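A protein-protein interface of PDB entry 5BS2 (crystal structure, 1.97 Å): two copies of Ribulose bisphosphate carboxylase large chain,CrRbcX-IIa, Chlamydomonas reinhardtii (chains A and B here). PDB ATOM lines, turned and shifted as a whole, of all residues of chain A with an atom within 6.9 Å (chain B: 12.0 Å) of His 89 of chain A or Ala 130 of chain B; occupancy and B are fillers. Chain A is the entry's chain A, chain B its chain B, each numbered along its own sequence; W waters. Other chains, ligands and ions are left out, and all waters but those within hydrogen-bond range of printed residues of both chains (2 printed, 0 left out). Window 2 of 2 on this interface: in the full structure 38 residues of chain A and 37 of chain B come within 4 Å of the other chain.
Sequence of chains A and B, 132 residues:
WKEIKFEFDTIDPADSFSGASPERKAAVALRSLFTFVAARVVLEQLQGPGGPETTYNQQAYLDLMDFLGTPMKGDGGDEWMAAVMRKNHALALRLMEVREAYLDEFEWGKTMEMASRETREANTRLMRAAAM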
ATOM      1  N   ASP A  63      -5.946 -20.731  32.903  1.00  0.00           N
ATOM      2  CA  ASP A  63      -4.971 -21.721  32.481  1.00  0.00           C
ATOM      3  C   ASP A  63      -3.755 -21.059  31.848  1.00  0.00           C
ATOM      4  O   ASP A  63      -2.617 -21.508  32.047  1.00  0.00           O
ATOM      5  CB  ASP A  63      -5.560 -22.692  31.459  1.00  0.00           C
ATOM      6  CG  ASP A  63      -6.672 -23.547  32.007  1.00  0.00           C
ATOM      7  OD1 ASP A  63      -6.685 -23.846  33.197  1.00  0.00           O
ATOM      8  OD2 ASP A  63      -7.553 -23.965  31.202  1.00  0.00           O
ATOM      9  N   VAL A  84      -0.217 -27.489  27.456  1.00  0.00           N
ATOM     10  CA  VAL A  84      -1.388 -26.620  27.441  1.00  0.00           C
ATOM     11  C   VAL A  84      -2.572 -27.338  26.810  1.00  0.00           C
ATOM     12  O   VAL A  84      -3.684 -27.271  27.331  1.00  0.00           O
ATOM     13  CB  VAL A  84      -1.177 -25.314  26.661  1.00  0.00           C
ATOM     14  CG1 VAL A  84      -2.486 -24.550  26.591  1.00  0.00           C
ATOM     15  CG2 VAL A  84      -0.130 -24.451  27.362  1.00  0.00           C
ATOM     16  N   MET A  85      -2.306 -28.041  25.714  1.00  0.00           N
ATOM     17  CA  MET A  85      -3.354 -28.741  24.983  1.00  0.00           C
ATOM     18  C   MET A  85      -4.035 -29.805  25.819  1.00  0.00           C
ATOM     19  O   MET A  85      -5.255 -29.968  25.704  1.00  0.00           O
ATOM     20  CB  MET A  85      -2.821 -29.381  23.707  1.00  0.00           C
ATOM     21  CG  MET A  85      -3.931 -29.845  22.753  1.00  0.00           C
ATOM     22  SD  MET A  85      -3.247 -30.178  21.122  1.00  0.00           S
ATOM     23  CE  MET A  85      -2.293 -31.617  21.551  1.00  0.00           C
ATOM     24  N   ARG A  86      -3.271 -30.519  26.654  1.00  0.00           N
ATOM     25  CA  ARG A  86      -3.852 -31.500  27.534  1.00  0.00           C
ATOM     26  C   ARG A  86      -4.829 -30.869  28.508  1.00  0.00           C
ATOM     27  O   ARG A  86      -5.904 -31.402  28.744  1.00  0.00           O
ATOM     28  CB  ARG A  86      -2.766 -32.288  28.270  1.00  0.00           C
ATOM     29  CG  ARG A  86      -2.109 -33.283  27.322  1.00  0.00           C
ATOM     30  CD  ARG A  86      -0.981 -34.094  27.941  1.00  0.00           C
ATOM     31  NE  ARG A  86       0.320 -33.694  27.380  1.00  0.00           N
ATOM     32  CZ  ARG A  86       1.392 -33.361  28.113  1.00  0.00           C
ATOM     33  NH1 ARG A  86       2.507 -32.992  27.499  1.00  0.00           N
ATOM     34  NH2 ARG A  86       1.372 -33.376  29.452  1.00  0.00           N
ATOM     35  N   LYS A  87      -4.454 -29.727  29.066  1.00  0.00           N
ATOM     36  CA  LYS A  87      -5.268 -29.032  30.059  1.00  0.00           C
ATOM     37  C   LYS A  87      -6.448 -28.287  29.413  1.00  0.00           C
ATOM     38  O   LYS A  87      -7.565 -28.332  29.917  1.00  0.00           O
ATOM     39  CB  LYS A  87      -4.397 -28.041  30.838  1.00  0.00           C
ATOM     40  CG  LYS A  87      -5.132 -27.319  31.956  1.00  0.00           C
ATOM     41  CD  LYS A  87      -5.654 -28.297  32.993  1.00  0.00           C
ATOM     42  CE  LYS A  87      -5.890 -27.616  34.341  1.00  0.00           C
ATOM     43  NZ  LYS A  87      -6.867 -26.493  34.161  1.00  0.00           N
ATOM     44  N   ASN A  88      -6.197 -27.624  28.288  1.00  0.00           N
ATOM     45  CA  ASN A  88      -7.206 -26.797  27.650  1.00  0.00           C
ATOM     46  C   ASN A  88      -6.999 -26.779  26.162  1.00  0.00           C
ATOM     47  O   ASN A  88      -6.195 -25.998  25.627  1.00  0.00           O
ATOM     48  CB  ASN A  88      -7.149 -25.360  28.224  1.00  0.00           C
ATOM     49  CG  ASN A  88      -8.358 -24.543  27.873  1.00  0.00           C
ATOM     50  OD1 ASN A  88      -8.937 -24.689  26.795  1.00  0.00           O
ATOM     51  ND2 ASN A  88      -8.754 -23.660  28.772  1.00  0.00           N
ATOM     52  N   HIS A  89      -7.726 -27.677  25.490  1.00  0.00           N
ATOM     53  CA  HIS A  89      -7.523 -27.902  24.086  1.00  0.00           C
ATOM     54  C   HIS A  89      -7.941 -26.692  23.298  1.00  0.00           C
ATOM     55  O   HIS A  89      -7.287 -26.356  22.313  1.00  0.00           O
ATOM     56  CB  HIS A  89      -8.339 -29.144  23.660  1.00  0.00           C
ATOM     57  CG  HIS A  89      -8.392 -29.368  22.195  1.00  0.00           C
ATOM     58  ND1 HIS A  89      -7.329 -29.892  21.487  1.00  0.00           N
ATOM     59  CD2 HIS A  89      -9.406 -29.226  21.300  1.00  0.00           C
ATOM     60  CE1 HIS A  89      -7.685 -30.056  20.215  1.00  0.00           C
ATOM     61  NE2 HIS A  89      -8.935 -29.656  20.084  1.00  0.00           N
ATOM     62  N   ALA A  90      -9.065 -26.080  23.670  1.00  0.00           N
ATOM     63  CA  ALA A  90      -9.521 -24.845  22.994  1.00  0.00           C
ATOM     64  C   ALA A  90      -8.455 -23.763  23.044  1.00  0.00           C
ATOM     65  O   ALA A  90      -8.188 -23.078  22.092  1.00  0.00           O
ATOM     66  CB  ALA A  90     -10.819 -24.334  23.628  1.00  0.00           C
ATOM     67  N   LEU A  91      -7.820 -23.617  24.201  1.00  0.00           N
ATOM     68  CA  LEU A  91      -6.764 -22.646  24.293  1.00  0.00           C
ATOM     69  C   LEU A  91      -5.581 -22.991  23.406  1.00  0.00           C
ATOM     70  O   LEU A  91      -5.048 -22.119  22.720  1.00  0.00           O
ATOM     71  CB  LEU A  91      -6.337 -22.508  25.764  1.00  0.00           C
ATOM     72  CG  LEU A  91      -5.173 -21.593  26.045  1.00  0.00           C
ATOM     73  CD1 LEU A  91      -5.486 -20.156  25.593  1.00  0.00           C
ATOM     74  CD2 LEU A  91      -4.839 -21.641  27.519  1.00  0.00           C
ATOM     75  N   ALA A  92      -5.180 -24.268  23.364  1.00  0.00           N
ATOM     76  CA  ALA A  92      -4.028 -24.635  22.577  1.00  0.00           C
ATOM     77  C   ALA A  92      -4.287 -24.350  21.101  1.00  0.00           C
ATOM     78  O   ALA A  92      -3.404 -23.843  20.369  1.00  0.00           O
ATOM     79  CB  ALA A  92      -3.663 -26.091  22.818  1.00  0.00           C
ATOM     80  N   LEU A  93      -5.492 -24.678  20.647  1.00  0.00           N
ATOM     81  CA  LEU A  93      -5.842 -24.414  19.252  1.00  0.00           C
ATOM     82  C   LEU A  93      -5.705 -22.953  18.893  1.00  0.00           C
ATOM     83  O   LEU A  93      -5.160 -22.634  17.850  1.00  0.00           O
ATOM     84  CB  LEU A  93      -7.266 -24.824  18.934  1.00  0.00           C
ATOM     85  CG  LEU A  93      -7.608 -26.303  18.857  1.00  0.00           C
ATOM     86  CD1 LEU A  93      -9.109 -26.453  18.562  1.00  0.00           C
ATOM     87  CD2 LEU A  93      -6.790 -27.013  17.784  1.00  0.00           C
ATOM     88  N   ARG A  94      -6.195 -22.071  19.766  1.00  0.00           N
ATOM     89  CA  ARG A  94      -6.061 -20.640  19.549  1.00  0.00           C
ATOM     90  C   ARG A  94      -4.591 -20.166  19.541  1.00  0.00           C
ATOM     91  O   ARG A  94      -4.180 -19.378  18.687  1.00  0.00           O
ATOM     92  CB  ARG A  94      -6.914 -19.853  20.573  1.00  0.00           C
ATOM     93  CG  ARG A  94      -6.858 -18.348  20.390  1.00  0.00           C
ATOM     94  CD  ARG A  94      -7.353 -17.898  19.026  1.00  0.00           C
ATOM     95  NE  ARG A  94      -7.316 -16.463  18.937  1.00  0.00           N
ATOM     96  CZ  ARG A  94      -7.272 -15.777  17.810  1.00  0.00           C
ATOM     97  NH1 ARG A  94      -7.358 -16.384  16.628  1.00  0.00           N
ATOM     98  NH2 ARG A  94      -7.203 -14.460  17.873  1.00  0.00           N
ATOM     99  N   MET A  96      -1.944 -21.952  18.865  1.00  0.00           N
ATOM    100  CA  MET A  96      -1.338 -22.463  17.636  1.00  0.00           C
ATOM    101  C   MET A  96      -1.765 -21.651  16.428  1.00  0.00           C
ATOM    102  O   MET A  96      -0.944 -21.390  15.543  1.00  0.00           O
ATOM    103  CB  MET A  96      -1.688 -23.930  17.426  1.00  0.00           C
ATOM    104  CG  MET A  96      -0.936 -24.823  18.370  1.00  0.00           C
ATOM    105  SD  MET A  96      -1.197 -26.589  18.106  1.00  0.00           S
ATOM    106  CE  MET A  96      -2.710 -26.843  19.007  1.00  0.00           C
ATOM    107  N   GLU B 121       4.262 -27.412  10.722  1.00  0.00           N
ATOM    108  CA  GLU B 121       4.323 -28.865  10.932  1.00  0.00           C
ATOM    109  C   GLU B 121       4.062 -29.309  12.387  1.00  0.00           C
ATOM    110  O   GLU B 121       3.374 -30.295  12.613  1.00  0.00           O
ATOM    111  CB  GLU B 121       5.650 -29.435  10.432  1.00  0.00           C
ATOM    112  CG  GLU B 121       5.811 -29.318   8.930  1.00  0.00           C
ATOM    113  CD  GLU B 121       7.142 -29.821   8.417  1.00  0.00           C
ATOM    114  OE1 GLU B 121       8.102 -29.977   9.209  1.00  0.00           O
ATOM    115  OE2 GLU B 121       7.226 -30.072   7.201  1.00  0.00           O
ATOM    116  N   ALA B 122       4.587 -28.567  13.379  1.00  0.00           N
ATOM    117  CA  ALA B 122       4.297 -28.899  14.787  1.00  0.00           C
ATOM    118  C   ALA B 122       2.810 -28.688  15.128  1.00  0.00           C
ATOM    119  O   ALA B 122       2.201 -29.530  15.776  1.00  0.00           O
ATOM    120  CB  ALA B 122       5.180 -28.111  15.709  1.00  0.00           C
ATOM    121  N   ASN B 123       2.225 -27.589  14.648  1.00  0.00           N
ATOM    122  CA  ASN B 123       0.803 -27.352  14.816  1.00  0.00           C
ATOM    123  C   ASN B 123      -0.024 -28.528  14.266  1.00  0.00           C
ATOM    124  O   ASN B 123      -0.954 -29.014  14.885  1.00  0.00           O
ATOM    125  CB  ASN B 123       0.387 -26.074  14.084  1.00  0.00           C
ATOM    126  CG  ASN B 123       0.701 -24.797  14.887  1.00  0.00           C
ATOM    127  OD1 ASN B 123       1.269 -24.849  15.953  1.00  0.00           O
ATOM    128  ND2 ASN B 123       0.335 -23.660  14.335  1.00  0.00           N
ATOM    129  N   THR B 124       0.351 -28.968  13.091  1.00  0.00           N
ATOM    130  CA  THR B 124      -0.378 -30.051  12.438  1.00  0.00           C
ATOM    131  C   THR B 124      -0.291 -31.350  13.228  1.00  0.00           C
ATOM    132  O   THR B 124      -1.272 -32.037  13.394  1.00  0.00           O
ATOM    133  CB  THR B 124       0.158 -30.264  11.032  1.00  0.00           C
ATOM    134  OG1 THR B 124      -0.049 -29.064  10.287  1.00  0.00           O
ATOM    135  CG2 THR B 124      -0.533 -31.441  10.350  1.00  0.00           C
ATOM    136  N   ARG B 125       0.892 -31.664  13.722  1.00  0.00           N
ATOM    137  CA  ARG B 125       1.088 -32.880  14.451  1.00  0.00           C
ATOM    138  C   ARG B 125       0.361 -32.839  15.800  1.00  0.00           C
ATOM    139  O   ARG B 125      -0.267 -33.825  16.211  1.00  0.00           O
ATOM    140  CB  ARG B 125       2.601 -33.151  14.543  1.00  0.00           C
ATOM    141  CG  ARG B 125       3.145 -33.497  15.925  1.00  0.00           C
ATOM    142  CD  ARG B 125       3.500 -34.961  16.131  1.00  0.00           C
ATOM    143  NE  ARG B 125       4.926 -35.270  15.916  1.00  0.00           N
ATOM    144  CZ  ARG B 125       5.642 -36.145  16.641  1.00  0.00           C
ATOM    145  NH1 ARG B 125       5.098 -36.778  17.670  1.00  0.00           N
ATOM    146  NH2 ARG B 125       6.933 -36.360  16.366  1.00  0.00           N
ATOM    147  N   LEU B 126       0.448 -31.702  16.489  1.00  0.00           N
ATOM    148  CA  LEU B 126      -0.275 -31.524  17.747  1.00  0.00           C
ATOM    149  C   LEU B 126      -1.800 -31.630  17.556  1.00  0.00           C
ATOM    150  O   LEU B 126      -2.470 -32.368  18.269  1.00  0.00           O
ATOM    151  CB  LEU B 126       0.098 -30.171  18.421  1.00  0.00           C
ATOM    152  CG  LEU B 126       1.481 -30.144  19.099  1.00  0.00           C
ATOM    153  CD1 LEU B 126       1.987 -28.738  19.354  1.00  0.00           C
ATOM    154  CD2 LEU B 126       1.462 -30.908  20.426  1.00  0.00           C
ATOM    155  N   MET B 127      -2.341 -30.914  16.588  1.00  0.00           N
ATOM    156  CA  MET B 127      -3.771 -30.957  16.324  1.00  0.00           C
ATOM    157  C   MET B 127      -4.243 -32.354  15.903  1.00  0.00           C
ATOM    158  O   MET B 127      -5.259 -32.852  16.413  1.00  0.00           O
ATOM    159  CB  MET B 127      -4.138 -29.941  15.243  1.00  0.00           C
ATOM    160  CG  MET B 127      -4.014 -28.514  15.716  1.00  0.00           C
ATOM    161  SD  MET B 127      -4.182 -27.318  14.382  1.00  0.00           S
ATOM    162  CE  MET B 127      -2.952 -26.106  14.813  1.00  0.00           C
ATOM    163  N   ARG B 128      -3.493 -32.996  15.002  1.00  0.00           N
ATOM    164  CA  ARG B 128      -3.840 -34.359  14.553  1.00  0.00           C
ATOM    165  C   ARG B 128      -3.883 -35.302  15.739  1.00  0.00           C
ATOM    166  O   ARG B 128      -4.806 -36.118  15.893  1.00  0.00           O
ATOM    167  CB  ARG B 128      -2.848 -34.844  13.506  1.00  0.00           C
ATOM    168  N   ALA B 129      -2.903 -35.174  16.622  1.00  0.00           N
ATOM    169  CA  ALA B 129      -2.852 -36.034  17.787  1.00  0.00           C
ATOM    170  C   ALA B 129      -4.085 -35.874  18.695  1.00  0.00           C
ATOM    171  O   ALA B 129      -4.626 -36.856  19.192  1.00  0.00           O
ATOM    172  CB  ALA B 129      -1.578 -35.752  18.551  1.00  0.00           C
ATOM    173  N   ALA B 130      -4.543 -34.628  18.889  1.00  0.00           N
ATOM    174  CA  ALA B 130      -5.642 -34.340  19.819  1.00  0.00           C
ATOM    175  C   ALA B 130      -7.013 -34.604  19.219  1.00  0.00           C
ATOM    176  O   ALA B 130      -7.984 -34.783  19.945  1.00  0.00           O
ATOM    177  CB  ALA B 130      -5.569 -32.898  20.283  1.00  0.00           C
ATOM    178  N   ALA B 131      -7.090 -34.609  17.894  1.00  0.00           N
ATOM    179  CA  ALA B 131      -8.354 -34.807  17.197  1.00  0.00           C
ATOM    180  C   ALA B 131      -8.866 -36.237  17.289  1.00  0.00           C
ATOM    181  O   ALA B 131      -8.115 -37.190  17.512  1.00  0.00           O
ATOM    182  CB  ALA B 131      -8.214 -34.424  15.735  1.00  0.00           C
ATOM    183  N   MET B 132     -10.169 -36.353  17.073  1.00  0.00           N
ATOM    184  CA  MET B 132     -10.898 -37.605  17.172  1.00  0.00           C
ATOM    185  C   MET B 132     -11.870 -37.819  16.009  1.00  0.00           C
ATOM    186  O   MET B 132     -12.367 -38.926  15.835  1.00  0.00           O
ATOM    187  CB  MET B 132     -11.708 -37.580  18.456  1.00  0.00           C
ATOM    188  CG  MET B 132     -11.056 -38.296  19.607  1.00  0.00           C
ATOM    189  SD  MET B 132     -11.703 -37.607  21.124  1.00  0.00           S
ATOM    190  CE  MET B 132     -10.572 -36.246  21.323  1.00  0.00           C
ATOM    191  OXT MET B 132     -12.217 -36.914  15.248  1.00  0.00           O
HETATM  192  O   HOH W   1      -5.305 -24.216  15.534  1.00  0.00           O
HETATM  193  O   HOH W   2      -7.252 -31.230  17.488  1.00  0.00           O
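No residue of chain B comes within 4 Å of Asn 88 of chain A. His 89 of chain A touches just one residue of chain B: Ala 130. No residue of chain B comes within 4 Å of Ala 90 of chain A. Of chain B, only Met 127 comes within 4 Å of Leu 93 of chain A. Of the printed residues of chain B, Met 96 of chain A touches Asn 123 (2.9 Å), Leu 126 (3.8 Å) and Met 127 (3.6 Å). Printed residues of chain A within 4 Å of Asn 123 of chain B: Met 96. Of the printed residues of chain A, Leu 126 of chain B touches Met 85 and Met 96. Printed residues of chain A within 4 Å of Met 127 of chain B: Leu 93 and Met 96. Of chain A, only Met 85 and His 89 come within 4 Å of Ala 130 of chain B. Ala 131 of chain B touches none of the printed residues of chain A. The nearest residue of chain B that does not touch His 89 of chain A is Ala 131 of chain B (5.1 Å). The nearest residue of chain A that does not touch Ala 130 of chain B is Leu 93 of chain A (6.5 Å). The nearest printed residue of chain A that does not touch Met 127 of chain B is Met 85 of chain A (4.7 Å).
O of Met 96 of chain A is in hydrogen-bond range of ND2 of Asn 123 of chain B. The side-chain sulfur (SD) of Met 85 of chain A lies close to the backbone carbonyl oxygen (O) of Leu 126 of chain B (3.7 Å).
Of the 13 printed residues of chain A, 4 touch a printed residue of chain B. Printed residues of chain A that touch a printed residue of chain B: Met 85, His 89, Leu 93 and Met 96. Hydrophobic or aromatic side chains of chain A that line the printed part of chain B: Met 85, His 89, Leu 93 and Met 96. Among the printed residues, no Asp or Glu carboxylate lies within 4 Å of a Lys or Arg side-chain nitrogen of the other chain.
Among the printed residues, pairs that only touch across the chains: Met 85 of chain A with Ala 130 of chain B (3.7 Å), His 89 of chain A with Ala 130 of chain B (3.5 Å), Leu 93 of chain A with Met 127 of chain B (3.8 Å), Met 96 of chain A with Leu 126 of chain B (3.8 Å) and Met 96 of chain A with Met 127 of chain B (3.6 Å).
Water W2 lies within hydrogen-bond range of O of Met 127 of chain B (2.8 Å), N of Ala 131 of chain B (3.4 Å) and NE2 of His 89 of chain A (3.5 Å). Water W1 bridges O of Leu 93 of chain A (2.8 Å) and SD of Met 127 of chain B (3.5 Å).
No position is printed for both chains. Of the 7 pairs that touch across the chains among the printed residues, none has its exchanged pair printed and touching as well.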
